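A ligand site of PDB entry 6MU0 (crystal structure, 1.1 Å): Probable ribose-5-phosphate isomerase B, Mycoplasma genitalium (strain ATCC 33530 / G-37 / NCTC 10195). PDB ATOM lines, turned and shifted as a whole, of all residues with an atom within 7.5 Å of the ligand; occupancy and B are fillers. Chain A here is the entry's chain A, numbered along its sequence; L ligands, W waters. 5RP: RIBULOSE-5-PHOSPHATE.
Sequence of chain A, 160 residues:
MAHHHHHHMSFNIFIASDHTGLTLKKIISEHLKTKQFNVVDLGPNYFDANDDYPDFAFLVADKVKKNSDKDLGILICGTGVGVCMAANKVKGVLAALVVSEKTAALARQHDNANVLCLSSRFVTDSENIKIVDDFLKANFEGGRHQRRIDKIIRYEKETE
N of Thr 79 lies within hydrogen-bond range of O4 of the ligand, 3.2 Å away. O11 of the ligand sits at hydrogen-bond distance from NE2 of His 19 (2.7 Å). The backbone NH (N) of Gly 78 is in hydrogen-bond range of an oxygen (O13) of the ligand. An oxygen (O1) of the ligand is in hydrogen-bond range of OD2 of CSD 77 (2.9 Å). The guanidinium group (NH2) of Arg 121 is in salt-bridge range of an oxygen (O11) of the ligand (2.9 Å). OD2 of Asp 18 sits at hydrogen-bond distance from O13 of the ligand (2.7 Å). An oxygen (O1) of the ligand sits at hydrogen-bond distance from the backbone NH (N) of Gly 82 (3.1 Å). The side-chain hydroxyl (OG1) of Thr 79 is in hydrogen-bond range of an oxygen (O1) of the ligand (3.3 Å).
The backbone NH (N) of Arg 121 lies within hydrogen-bond range of the backbone carbonyl oxygen (O) of Gly 78 (3.0 Å). The side-chain carboxylate (OD1) of Asp 18 lies within hydrogen-bond range of the side-chain hydroxyl (OG1) of Thr 20, at 2.7 Å. OD1 of CSD 77 lies within hydrogen-bond range of the backbone NH of Gly 82, at 3.1 Å. The backbone NH of Asp 18 lies within hydrogen-bond range of the backbone carbonyl oxygen of Ile 76 (3.2 Å). N of Gly 80 sits at hydrogen-bond distance from OD2 of CSD 77 (2.7 Å). The side-chain hydroxyl (OG1) of Thr 20 lies within hydrogen-bond range of the side-chain hydroxyl (OG) of Ser 120. OD1 of CSD 77 sits at hydrogen-bond distance from the backbone NH (N) of Val 83 (2.8 Å). The backbone NH (N) of Val 81 lies within hydrogen-bond range of the side-chain hydroxyl (OG1) of Thr 79 (3.2 Å).
Residues that only touch the ligand: Thr 20 and Tyr 53. The nearest printed residue that does not touch the ligand is Val 81 (4.02 Å).
Water W2 bridges an oxygen (O12) of the ligand (2.6 Å) and the guanidinium group (NH2) of Arg 121 (3.5 Å). Water W4 bridges O10 of the ligand (2.6 Å) and O of Ala 49 (2.8 Å). Water W5 lies within hydrogen-bond range of an oxygen (O11) of the ligand (2.8 Å), the backbone carbonyl oxygen (O) of Ala 49 (2.9 Å) and a ring nitrogen (NE2) of His 19 (3.3 Å).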
ATOM      1  N   ASP A  18     -28.999   1.047  23.649  1.00  0.00           N
ATOM      2  CA  ASP A  18     -29.588   1.639  24.841  1.00  0.00           C
ATOM      3  C   ASP A  18     -30.906   2.316  24.457  1.00  0.00           C
ATOM      4  O   ASP A  18     -31.417   2.159  23.343  1.00  0.00           O
ATOM      5  CB  ASP A  18     -28.612   2.556  25.575  1.00  0.00           C
ATOM      6  CG  ASP A  18     -28.337   3.875  24.853  1.00  0.00           C
ATOM      7  OD1 ASP A  18     -28.828   4.057  23.716  1.00  0.00           O
ATOM      8  OD2 ASP A  18     -27.614   4.715  25.440  1.00  0.00           O
ATOM      9  N   HIS A  19     -31.462   3.076  25.406  1.00  0.00           N
ATOM     10  CA  HIS A  19     -32.735   3.744  25.212  1.00  0.00           C
ATOM     11  C   HIS A  19     -32.769   4.665  24.009  1.00  0.00           C
ATOM     12  O   HIS A  19     -33.866   5.010  23.551  1.00  0.00           O
ATOM     13  CB  HIS A  19     -33.087   4.573  26.453  1.00  0.00           C
ATOM     14  CG  HIS A  19     -32.018   5.549  26.847  1.00  0.00           C
ATOM     15  ND1 HIS A  19     -31.009   5.237  27.735  1.00  0.00           N
ATOM     16  CD2 HIS A  19     -31.799   6.838  26.474  1.00  0.00           C
ATOM     17  CE1 HIS A  19     -30.218   6.279  27.892  1.00  0.00           C
ATOM     18  NE2 HIS A  19     -30.679   7.266  27.137  1.00  0.00           N
ATOM     19  N   THR A  20     -31.610   5.101  23.489  1.00  0.00           N
ATOM     20  CA  THR A  20     -31.615   6.041  22.376  1.00  0.00           C
ATOM     21  C   THR A  20     -31.905   5.370  21.040  1.00  0.00           C
ATOM     22  O   THR A  20     -32.135   6.074  20.053  1.00  0.00           O
ATOM     23  CB  THR A  20     -30.275   6.784  22.248  1.00  0.00           C
ATOM     24  OG1 THR A  20     -29.265   5.882  21.772  1.00  0.00           O
ATOM     25  CG2 THR A  20     -29.834   7.399  23.566  1.00  0.00           C
ATOM     26  N   GLY A  21     -31.861   4.041  20.971  1.00  0.00           N
ATOM     27  CA  GLY A  21     -31.820   3.385  19.681  1.00  0.00           C
ATOM     28  C   GLY A  21     -32.888   2.362  19.388  1.00  0.00           C
ATOM     29  O   GLY A  21     -32.695   1.522  18.506  1.00  0.00           O
ATOM     30  N   PHE A  47     -38.865   1.300  26.445  1.00  0.00           N
ATOM     31  CA  PHE A  47     -38.068   2.508  26.637  1.00  0.00           C
ATOM     32  C   PHE A  47     -37.893   2.835  28.126  1.00  0.00           C
ATOM     33  O   PHE A  47     -38.869   2.929  28.875  1.00  0.00           O
ATOM     34  CB  PHE A  47     -38.742   3.683  25.935  1.00  0.00           C
ATOM     35  CG  PHE A  47     -37.983   4.970  26.087  1.00  0.00           C
ATOM     36  CD1 PHE A  47     -36.859   5.215  25.321  1.00  0.00           C
ATOM     37  CD2 PHE A  47     -38.391   5.925  27.004  1.00  0.00           C
ATOM     38  CE1 PHE A  47     -36.154   6.404  25.457  1.00  0.00           C
ATOM     39  CE2 PHE A  47     -37.689   7.106  27.155  1.00  0.00           C
ATOM     40  CZ  PHE A  47     -36.563   7.339  26.377  1.00  0.00           C
ATOM     41  N   ASP A  48     -36.638   3.034  28.511  1.00  0.00           N
ATOM     42  CA  ASP A  48     -36.259   3.515  29.845  1.00  0.00           C
ATOM     43  C   ASP A  48     -35.224   4.596  29.617  1.00  0.00           C
ATOM     44  O   ASP A  48     -34.072   4.289  29.297  1.00  0.00           O
ATOM     45  CB  ASP A  48     -35.686   2.375  30.677  1.00  0.00           C
ATOM     46  CG  ASP A  48     -35.108   2.839  32.018  1.00  0.00           C
ATOM     47  OD1 ASP A  48     -35.084   4.048  32.305  1.00  0.00           O
ATOM     48  OD2 ASP A  48     -34.656   1.965  32.785  1.00  0.00           O
ATOM     49  N   ALA A  49     -35.618   5.861  29.804  1.00  0.00           N
ATOM     50  CA  ALA A  49     -34.776   7.008  29.476  1.00  0.00           C
ATOM     51  C   ALA A  49     -33.420   6.964  30.174  1.00  0.00           C
ATOM     52  O   ALA A  49     -32.496   7.653  29.730  1.00  0.00           O
ATOM     53  CB  ALA A  49     -35.483   8.305  29.859  1.00  0.00           C
ATOM     54  N   ASN A  50     -33.298   6.212  31.265  1.00  0.00           N
ATOM     55  CA  ASN A  50     -32.084   6.207  32.086  1.00  0.00           C
ATOM     56  C   ASN A  50     -31.234   4.956  31.930  1.00  0.00           C
ATOM     57  O   ASN A  50     -30.242   4.828  32.658  1.00  0.00           O
ATOM     58  CB  ASN A  50     -32.466   6.420  33.548  1.00  0.00           C
ATOM     59  CG  ASN A  50     -33.336   7.625  33.721  1.00  0.00           C
ATOM     60  OD1 ASN A  50     -32.991   8.707  33.247  1.00  0.00           O
ATOM     61  ND2 ASN A  50     -34.501   7.434  34.328  1.00  0.00           N
ATOM     62  N   ASP A  51     -31.583   4.043  31.033  1.00  0.00           N
ATOM     63  CA  ASP A  51     -30.841   2.776  30.992  1.00  0.00           C
ATOM     64  C   ASP A  51     -29.425   2.964  30.464  1.00  0.00           C
ATOM     65  O   ASP A  51     -29.070   4.016  29.923  1.00  0.00           O
ATOM     66  CB  ASP A  51     -31.649   1.639  30.324  1.00  0.00           C
ATOM     67  CG  ASP A  51     -31.795   1.782  28.809  1.00  0.00           C
ATOM     68  OD1 ASP A  51     -31.102   2.600  28.178  1.00  0.00           O
ATOM     69  OD2 ASP A  51     -32.621   1.018  28.266  1.00  0.00           O
ATOM     70  N   ASP A  52     -28.612   1.931  30.640  1.00  0.00           N
ATOM     71  CA  ASP A  52     -27.153   2.053  30.578  1.00  0.00           C
ATOM     72  C   ASP A  52     -26.593   1.199  29.448  1.00  0.00           C
ATOM     73  O   ASP A  52     -26.645  -0.032  29.515  1.00  0.00           O
ATOM     74  CB  ASP A  52     -26.527   1.610  31.906  1.00  0.00           C
ATOM     75  CG  ASP A  52     -26.842   2.547  33.065  1.00  0.00           C
ATOM     76  OD1 ASP A  52     -27.314   3.684  32.837  1.00  0.00           O
ATOM     77  OD2 ASP A  52     -26.592   2.136  34.216  1.00  0.00           O
ATOM     78  N   TYR A  53     -26.004   1.847  28.447  1.00  0.00           N
ATOM     79  CA  TYR A  53     -25.479   1.134  27.284  1.00  0.00           C
ATOM     80  C   TYR A  53     -24.506  -0.006  27.611  1.00  0.00           C
ATOM     81  O   TYR A  53     -24.527  -1.000  26.867  1.00  0.00           O
ATOM     82  CB  TYR A  53     -24.875   2.099  26.240  1.00  0.00           C
ATOM     83  CG  TYR A  53     -23.653   2.805  26.764  1.00  0.00           C
ATOM     84  CD1 TYR A  53     -22.398   2.214  26.683  1.00  0.00           C
ATOM     85  CD2 TYR A  53     -23.770   4.032  27.408  1.00  0.00           C
ATOM     86  CE1 TYR A  53     -21.288   2.822  27.231  1.00  0.00           C
ATOM     87  CE2 TYR A  53     -22.659   4.659  27.953  1.00  0.00           C
ATOM     88  CZ  TYR A  53     -21.417   4.048  27.859  1.00  0.00           C
ATOM     89  OH  TYR A  53     -20.294   4.645  28.410  1.00  0.00           O
ATOM     90  N   PRO A  54     -23.641   0.048  28.639  1.00  0.00           N
ATOM     91  CA  PRO A  54     -22.739  -1.102  28.833  1.00  0.00           C
ATOM     92  C   PRO A  54     -23.472  -2.404  29.056  1.00  0.00           C
ATOM     93  O   PRO A  54     -22.991  -3.455  28.622  1.00  0.00           O
ATOM     94  CB  PRO A  54     -21.916  -0.705  30.065  1.00  0.00           C
ATOM     95  CG  PRO A  54     -21.938   0.764  30.061  1.00  0.00           C
ATOM     96  CD  PRO A  54     -23.338   1.117  29.608  1.00  0.00           C
ATOM     97  N   ILE A  76     -26.020  -0.129  19.198  1.00  0.00           N
ATOM     98  CA  ILE A  76     -26.459   1.230  18.907  1.00  0.00           C
ATOM     99  C   ILE A  76     -26.494   2.067  20.193  1.00  0.00           C
ATOM    100  O   ILE A  76     -27.067   1.650  21.193  1.00  0.00           O
ATOM    101  CB  ILE A  76     -27.876   1.229  18.293  1.00  0.00           C
ATOM    102  CG1 ILE A  76     -27.927   0.437  16.979  1.00  0.00           C
ATOM    103  CG2 ILE A  76     -28.395   2.639  18.105  1.00  0.00           C
ATOM    104  CD1 ILE A  76     -29.297  -0.191  16.716  1.00  0.00           C
ATOM    105  N   CSD A  77     -25.901   3.263  20.150  1.00  0.00           N
ATOM    106  CA  CSD A  77     -26.081   4.235  21.211  1.00  0.00           C
ATOM    107  CB  CSD A  77     -25.142   4.009  22.401  1.00  0.00           C
ATOM    108  SG  CSD A  77     -23.418   4.149  22.026  1.00  0.00           S
ATOM    109  C   CSD A  77     -26.006   5.626  20.589  1.00  0.00           C
ATOM    110  O   CSD A  77     -25.875   5.741  19.371  1.00  0.00           O
ATOM    111  OD1 CSD A  77     -22.784   3.821  23.316  1.00  0.00           O
ATOM    112  OD2 CSD A  77     -23.249   5.788  21.826  1.00  0.00           O
ATOM    113  N   GLY A  78     -26.105   6.690  21.390  1.00  0.00           N
ATOM    114  CA  GLY A  78     -26.156   8.044  20.861  1.00  0.00           C
ATOM    115  C   GLY A  78     -25.116   8.347  19.783  1.00  0.00           C
ATOM    116  O   GLY A  78     -25.466   8.837  18.698  1.00  0.00           O
ATOM    117  N   THR A  79     -23.850   8.058  20.081  1.00  0.00           N
ATOM    118  CA  THR A  79     -22.753   8.314  19.149  1.00  0.00           C
ATOM    119  C   THR A  79     -22.097   7.043  18.617  1.00  0.00           C
ATOM    120  O   THR A  79     -21.343   7.123  17.645  1.00  0.00           O
ATOM    121  CB  THR A  79     -21.654   9.133  19.839  1.00  0.00           C
ATOM    122  OG1 THR A  79     -21.185   8.385  20.967  1.00  0.00           O
ATOM    123  CG2 THR A  79     -22.145  10.518  20.260  1.00  0.00           C
ATOM    124  N   GLY A  80     -22.359   5.892  19.245  1.00  0.00           N
ATOM    125  CA  GLY A  80     -21.635   4.660  18.993  1.00  0.00           C
ATOM    126  C   GLY A  80     -20.422   4.449  19.864  1.00  0.00           C
ATOM    127  O   GLY A  80     -19.901   3.335  19.909  1.00  0.00           O
ATOM    128  N   VAL A  81     -19.944   5.478  20.565  1.00  0.00           N
ATOM    129  CA  VAL A  81     -18.664   5.391  21.270  1.00  0.00           C
ATOM    130  C   VAL A  81     -18.730   4.435  22.446  1.00  0.00           C
ATOM    131  O   VAL A  81     -17.833   3.608  22.636  1.00  0.00           O
ATOM    132  CB  VAL A  81     -18.202   6.783  21.712  1.00  0.00           C
ATOM    133  CG1 VAL A  81     -17.031   6.671  22.693  1.00  0.00           C
ATOM    134  CG2 VAL A  81     -17.824   7.628  20.518  1.00  0.00           C
ATOM    135  N   GLY A  82     -19.755   4.576  23.290  1.00  0.00           N
ATOM    136  CA  GLY A  82     -19.790   3.817  24.530  1.00  0.00           C
ATOM    137  C   GLY A  82     -19.873   2.317  24.304  1.00  0.00           C
ATOM    138  O   GLY A  82     -19.127   1.549  24.916  1.00  0.00           O
ATOM    139  N   VAL A  83     -20.783   1.893  23.430  1.00  0.00           N
ATOM    140  CA  VAL A  83     -20.892   0.468  23.131  1.00  0.00           C
ATOM    141  C   VAL A  83     -19.625  -0.055  22.485  1.00  0.00           C
ATOM    142  O   VAL A  83     -19.270  -1.226  22.677  1.00  0.00           O
ATOM    143  CB  VAL A  83     -22.142   0.157  22.271  1.00  0.00           C
ATOM    144  CG1 VAL A  83     -23.421   0.461  23.026  1.00  0.00           C
ATOM    145  CG2 VAL A  83     -22.082   0.888  20.916  1.00  0.00           C
ATOM    146  N   CYS A  84     -18.921   0.786  21.722  1.00  0.00           N
ATOM    147  CA  CYS A  84     -17.661   0.360  21.111  1.00  0.00           C
ATOM    148  C   CYS A  84     -16.581   0.144  22.164  1.00  0.00           C
ATOM    149  O   CYS A  84     -15.858  -0.869  22.120  1.00  0.00           O
ATOM    150  CB  CYS A  84     -17.238   1.391  20.057  1.00  0.00           C
ATOM    151  SG  CYS A  84     -15.732   1.030  19.181  1.00  0.00           S
ATOM    152  N   MET A  85     -16.441   1.083  23.110  1.00  0.00           N
ATOM    153  CA  MET A  85     -15.496   0.905  24.207  1.00  0.00           C
ATOM    154  C   MET A  85     -15.784  -0.377  24.972  1.00  0.00           C
ATOM    155  O   MET A  85     -14.887  -1.183  25.246  1.00  0.00           O
ATOM    156  CB  MET A  85     -15.616   2.056  25.201  1.00  0.00           C
ATOM    157  CG  MET A  85     -15.151   3.410  24.723  1.00  0.00           C
ATOM    158  SD  MET A  85     -15.552   4.631  25.986  1.00  0.00           S
ATOM    159  CE  MET A  85     -14.675   6.072  25.369  1.00  0.00           C
ATOM    160  N   LEU A 118     -23.011   1.736  15.981  1.00  0.00           N
ATOM    161  CA  LEU A 118     -23.736   2.736  15.216  1.00  0.00           C
ATOM    162  C   LEU A 118     -24.243   3.843  16.145  1.00  0.00           C
ATOM    163  O   LEU A 118     -24.513   3.615  17.335  1.00  0.00           O
ATOM    164  CB  LEU A 118     -24.966   2.122  14.533  1.00  0.00           C
ATOM    165  CG  LEU A 118     -24.706   0.929  13.626  1.00  0.00           C
ATOM    166  CD1 LEU A 118     -26.020   0.327  13.136  1.00  0.00           C
ATOM    167  CD2 LEU A 118     -23.830   1.316  12.450  1.00  0.00           C
ATOM    168  N   SER A 119     -24.410   5.016  15.550  1.00  0.00           N
ATOM    169  CA  SER A 119     -24.950   6.192  16.203  1.00  0.00           C
ATOM    170  C   SER A 119     -26.438   6.342  15.924  1.00  0.00           C
ATOM    171  O   SER A 119     -26.862   6.383  14.761  1.00  0.00           O
ATOM    172  CB  SER A 119     -24.230   7.424  15.662  1.00  0.00           C
ATOM    173  OG  SER A 119     -24.850   8.628  16.087  1.00  0.00           O
ATOM    174  N   SER A 120     -27.235   6.500  16.984  1.00  0.00           N
ATOM    175  CA  SER A 120     -28.648   6.785  16.865  1.00  0.00           C
ATOM    176  C   SER A 120     -28.966   8.267  16.751  1.00  0.00           C
ATOM    177  O   SER A 120     -30.028   8.619  16.218  1.00  0.00           O
ATOM    178  CB  SER A 120     -29.392   6.251  18.092  1.00  0.00           C
ATOM    179  OG  SER A 120     -28.877   6.889  19.245  1.00  0.00           O
ATOM    180  N   ARG A 121     -28.094   9.152  17.241  1.00  0.00           N
ATOM    181  CA  ARG A 121     -28.393  10.577  17.326  1.00  0.00           C
ATOM    182  C   ARG A 121     -27.779  11.400  16.210  1.00  0.00           C
ATOM    183  O   ARG A 121     -28.212  12.536  16.003  1.00  0.00           O
ATOM    184  CB  ARG A 121     -27.939  11.144  18.675  1.00  0.00           C
ATOM    185  CG  ARG A 121     -28.859  10.777  19.819  1.00  0.00           C
ATOM    186  CD  ARG A 121     -28.316  11.254  21.160  1.00  0.00           C
ATOM    187  NE  ARG A 121     -29.313  11.095  22.210  1.00  0.00           N
ATOM    188  CZ  ARG A 121     -29.044  10.891  23.494  1.00  0.00           C
ATOM    189  NH1 ARG A 121     -27.794  10.781  23.915  1.00  0.00           N
ATOM    190  NH2 ARG A 121     -30.052  10.800  24.352  1.00  0.00           N
ATOM    191  N   PHE A 122     -26.788  10.863  15.491  1.00  0.00           N
ATOM    192  CA  PHE A 122     -26.012  11.653  14.544  1.00  0.00           C
ATOM    193  C   PHE A 122     -26.001  11.086  13.136  1.00  0.00           C
ATOM    194  O   PHE A 122     -25.398  11.686  12.239  1.00  0.00           O
ATOM    195  CB  PHE A 122     -24.579  11.842  15.062  1.00  0.00           C
ATOM    196  CG  PHE A 122     -24.526  12.712  16.271  1.00  0.00           C
ATOM    197  CD1 PHE A 122     -24.439  14.095  16.145  1.00  0.00           C
ATOM    198  CD2 PHE A 122     -24.604  12.165  17.553  1.00  0.00           C
ATOM    199  CE1 PHE A 122     -24.414  14.902  17.243  1.00  0.00           C
ATOM    200  CE2 PHE A 122     -24.588  12.995  18.668  1.00  0.00           C
ATOM    201  CZ  PHE A 122     -24.496  14.364  18.516  1.00  0.00           C
HETATM  202  C2  5RP L   1     -22.738   6.685  24.759  1.00  0.00           C
HETATM  203  C3  5RP L   1     -23.999   7.342  24.250  1.00  0.00           C
HETATM  204  C5  5RP L   1     -25.283   7.139  25.078  1.00  0.00           C
HETATM  205  O13 5RP L   1     -26.345   6.715  24.250  1.00  0.00           O
HETATM  206  C6  5RP L   1     -25.563   8.518  25.680  1.00  0.00           C
HETATM  207  O14 5RP L   1     -24.444   8.895  26.494  1.00  0.00           O
HETATM  208  C7  5RP L   1     -26.836   8.546  26.497  1.00  0.00           C
HETATM  209  O8  5RP L   1     -27.122   9.918  26.810  1.00  0.00           O
HETATM  210  P9  5RP L   1     -28.397  10.272  27.718  1.00  0.00           P
HETATM  211  O12 5RP L   1     -28.400  11.763  27.822  1.00  0.00           O
HETATM  212  O11 5RP L   1     -29.630   9.724  26.996  1.00  0.00           O
HETATM  213  O10 5RP L   1     -28.221   9.567  29.051  1.00  0.00           O
HETATM  214  O4  5RP L   1     -24.028   8.048  23.268  1.00  0.00           O
HETATM  215  O1  5RP L   1     -21.637   6.970  23.897  1.00  0.00           O
HETATM  216  O   HOH W   1     -22.774  10.635  23.722  1.00  0.00           O
HETATM  217  O   HOH W   2     -29.874  13.498  26.572  1.00  0.00           O
HETATM  218  O   HOH W   3     -27.360  13.706  25.950  1.00  0.00           O
HETATM  219  O   HOH W   4     -30.158   8.854  30.646  1.00  0.00           O
HETATM  220  O   HOH W   5     -32.124  10.043  28.110  1.00  0.00           O
